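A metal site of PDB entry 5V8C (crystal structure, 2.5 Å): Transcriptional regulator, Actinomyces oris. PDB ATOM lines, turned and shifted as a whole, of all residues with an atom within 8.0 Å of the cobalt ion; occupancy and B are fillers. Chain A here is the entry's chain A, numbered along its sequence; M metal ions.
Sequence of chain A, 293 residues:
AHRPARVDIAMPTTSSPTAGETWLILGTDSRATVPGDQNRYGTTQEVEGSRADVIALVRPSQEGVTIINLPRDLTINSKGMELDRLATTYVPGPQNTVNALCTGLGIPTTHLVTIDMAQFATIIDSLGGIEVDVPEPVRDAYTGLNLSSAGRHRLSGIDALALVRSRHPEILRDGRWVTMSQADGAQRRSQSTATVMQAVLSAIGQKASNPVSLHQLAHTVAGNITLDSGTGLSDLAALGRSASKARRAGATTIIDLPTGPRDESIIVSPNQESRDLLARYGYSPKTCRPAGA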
ATOM      1  N   ALA A   1     -13.011 -28.143 -22.684  1.00  0.00           N
ATOM      2  CA  ALA A   1     -13.328 -29.250 -21.788  1.00  0.00           C
ATOM      3  C   ALA A   1     -12.140 -29.778 -20.952  1.00  0.00           C
ATOM      4  O   ALA A   1     -12.363 -30.339 -19.870  1.00  0.00           O
ATOM      5  CB  ALA A   1     -13.961 -30.394 -22.568  1.00  0.00           C
ATOM      6  N   HIS A   2     -10.887 -29.633 -21.456  1.00  0.00           N
ATOM      7  CA  HIS A   2      -9.627 -30.103 -20.846  1.00  0.00           C
ATOM      8  C   HIS A   2      -9.602 -30.247 -19.324  1.00  0.00           C
ATOM      9  O   HIS A   2      -9.674 -29.247 -18.603  1.00  0.00           O
ATOM     10  CB  HIS A   2      -8.449 -29.216 -21.281  1.00  0.00           C
ATOM     11  CG  HIS A   2      -8.044 -29.392 -22.703  1.00  0.00           C
ATOM     12  ND1 HIS A   2      -8.421 -28.471 -23.675  1.00  0.00           N
ATOM     13  CD2 HIS A   2      -7.314 -30.373 -23.284  1.00  0.00           C
ATOM     14  CE1 HIS A   2      -7.917 -28.926 -24.802  1.00  0.00           C
ATOM     15  NE2 HIS A   2      -7.243 -30.059 -24.626  1.00  0.00           N
ATOM     16  N   ARG A   3      -9.426 -31.487 -18.838  1.00  0.00           N
ATOM     17  CA  ARG A   3      -9.299 -31.804 -17.407  1.00  0.00           C
ATOM     18  C   ARG A   3      -7.994 -32.582 -17.175  1.00  0.00           C
ATOM     19  O   ARG A   3      -7.620 -33.394 -18.013  1.00  0.00           O
ATOM     20  CB  ARG A   3     -10.491 -32.648 -16.927  1.00  0.00           C
ATOM     21  CG  ARG A   3     -11.737 -31.839 -16.552  1.00  0.00           C
ATOM     22  CD  ARG A   3     -12.877 -32.742 -16.128  1.00  0.00           C
ATOM     23  NE  ARG A   3     -13.444 -33.484 -17.258  1.00  0.00           N
ATOM     24  CZ  ARG A   3     -14.097 -34.636 -17.152  1.00  0.00           C
ATOM     25  NH1 ARG A   3     -14.263 -35.206 -15.966  1.00  0.00           N
ATOM     26  NH2 ARG A   3     -14.579 -35.232 -18.226  1.00  0.00           N
ATOM     27  N   HIS A 219      -6.130 -23.519 -20.122  1.00  0.00           N
ATOM     28  CA  HIS A 219      -7.009 -24.620 -20.471  1.00  0.00           C
ATOM     29  C   HIS A 219      -6.209 -25.807 -21.032  1.00  0.00           C
ATOM     30  O   HIS A 219      -6.361 -26.909 -20.521  1.00  0.00           O
ATOM     31  CB  HIS A 219      -8.100 -24.177 -21.449  1.00  0.00           C
ATOM     32  CG  HIS A 219      -9.154 -25.199 -21.668  1.00  0.00           C
ATOM     33  ND1 HIS A 219     -10.049 -25.542 -20.665  1.00  0.00           N
ATOM     34  CD2 HIS A 219      -9.425 -25.951 -22.768  1.00  0.00           C
ATOM     35  CE1 HIS A 219     -10.813 -26.488 -21.176  1.00  0.00           C
ATOM     36  NE2 HIS A 219     -10.476 -26.768 -22.438  1.00  0.00           N
ATOM     37  N   THR A 220      -5.297 -25.564 -22.003  1.00  0.00           N
ATOM     38  CA  THR A 220      -4.472 -26.613 -22.615  1.00  0.00           C
ATOM     39  C   THR A 220      -3.502 -27.252 -21.625  1.00  0.00           C
ATOM     40  O   THR A 220      -3.359 -28.475 -21.635  1.00  0.00           O
ATOM     41  CB  THR A 220      -3.765 -26.130 -23.879  1.00  0.00           C
ATOM     42  OG1 THR A 220      -3.215 -24.839 -23.643  1.00  0.00           O
ATOM     43  CG2 THR A 220      -4.702 -26.087 -25.082  1.00  0.00           C
ATOM     44  N   GLY A 223      -5.184 -29.851 -19.475  1.00  0.00           N
ATOM     45  CA  GLY A 223      -5.471 -31.070 -20.232  1.00  0.00           C
ATOM     46  C   GLY A 223      -4.242 -31.867 -20.644  1.00  0.00           C
ATOM     47  O   GLY A 223      -4.387 -32.957 -21.179  1.00  0.00           O
HETATM   48 CO    CO M   1     -11.057 -28.876 -23.367  1.00  0.00          CO
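Of the 6 residues printed, 3 come within 4 Å of the cobalt ion.
Along chain A the residues within 4 Å of the cobalt ion span positions 1 to 219.
The cobalt ion is bound by N of His 2 (2.1 Å), N of Ala 1 (2.2 Å) and NE2 of His 219 (2.4 Å).
Slightly farther from the cobalt ion lies a ring nitrogen (ND1) of His 2 (2.7 Å).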
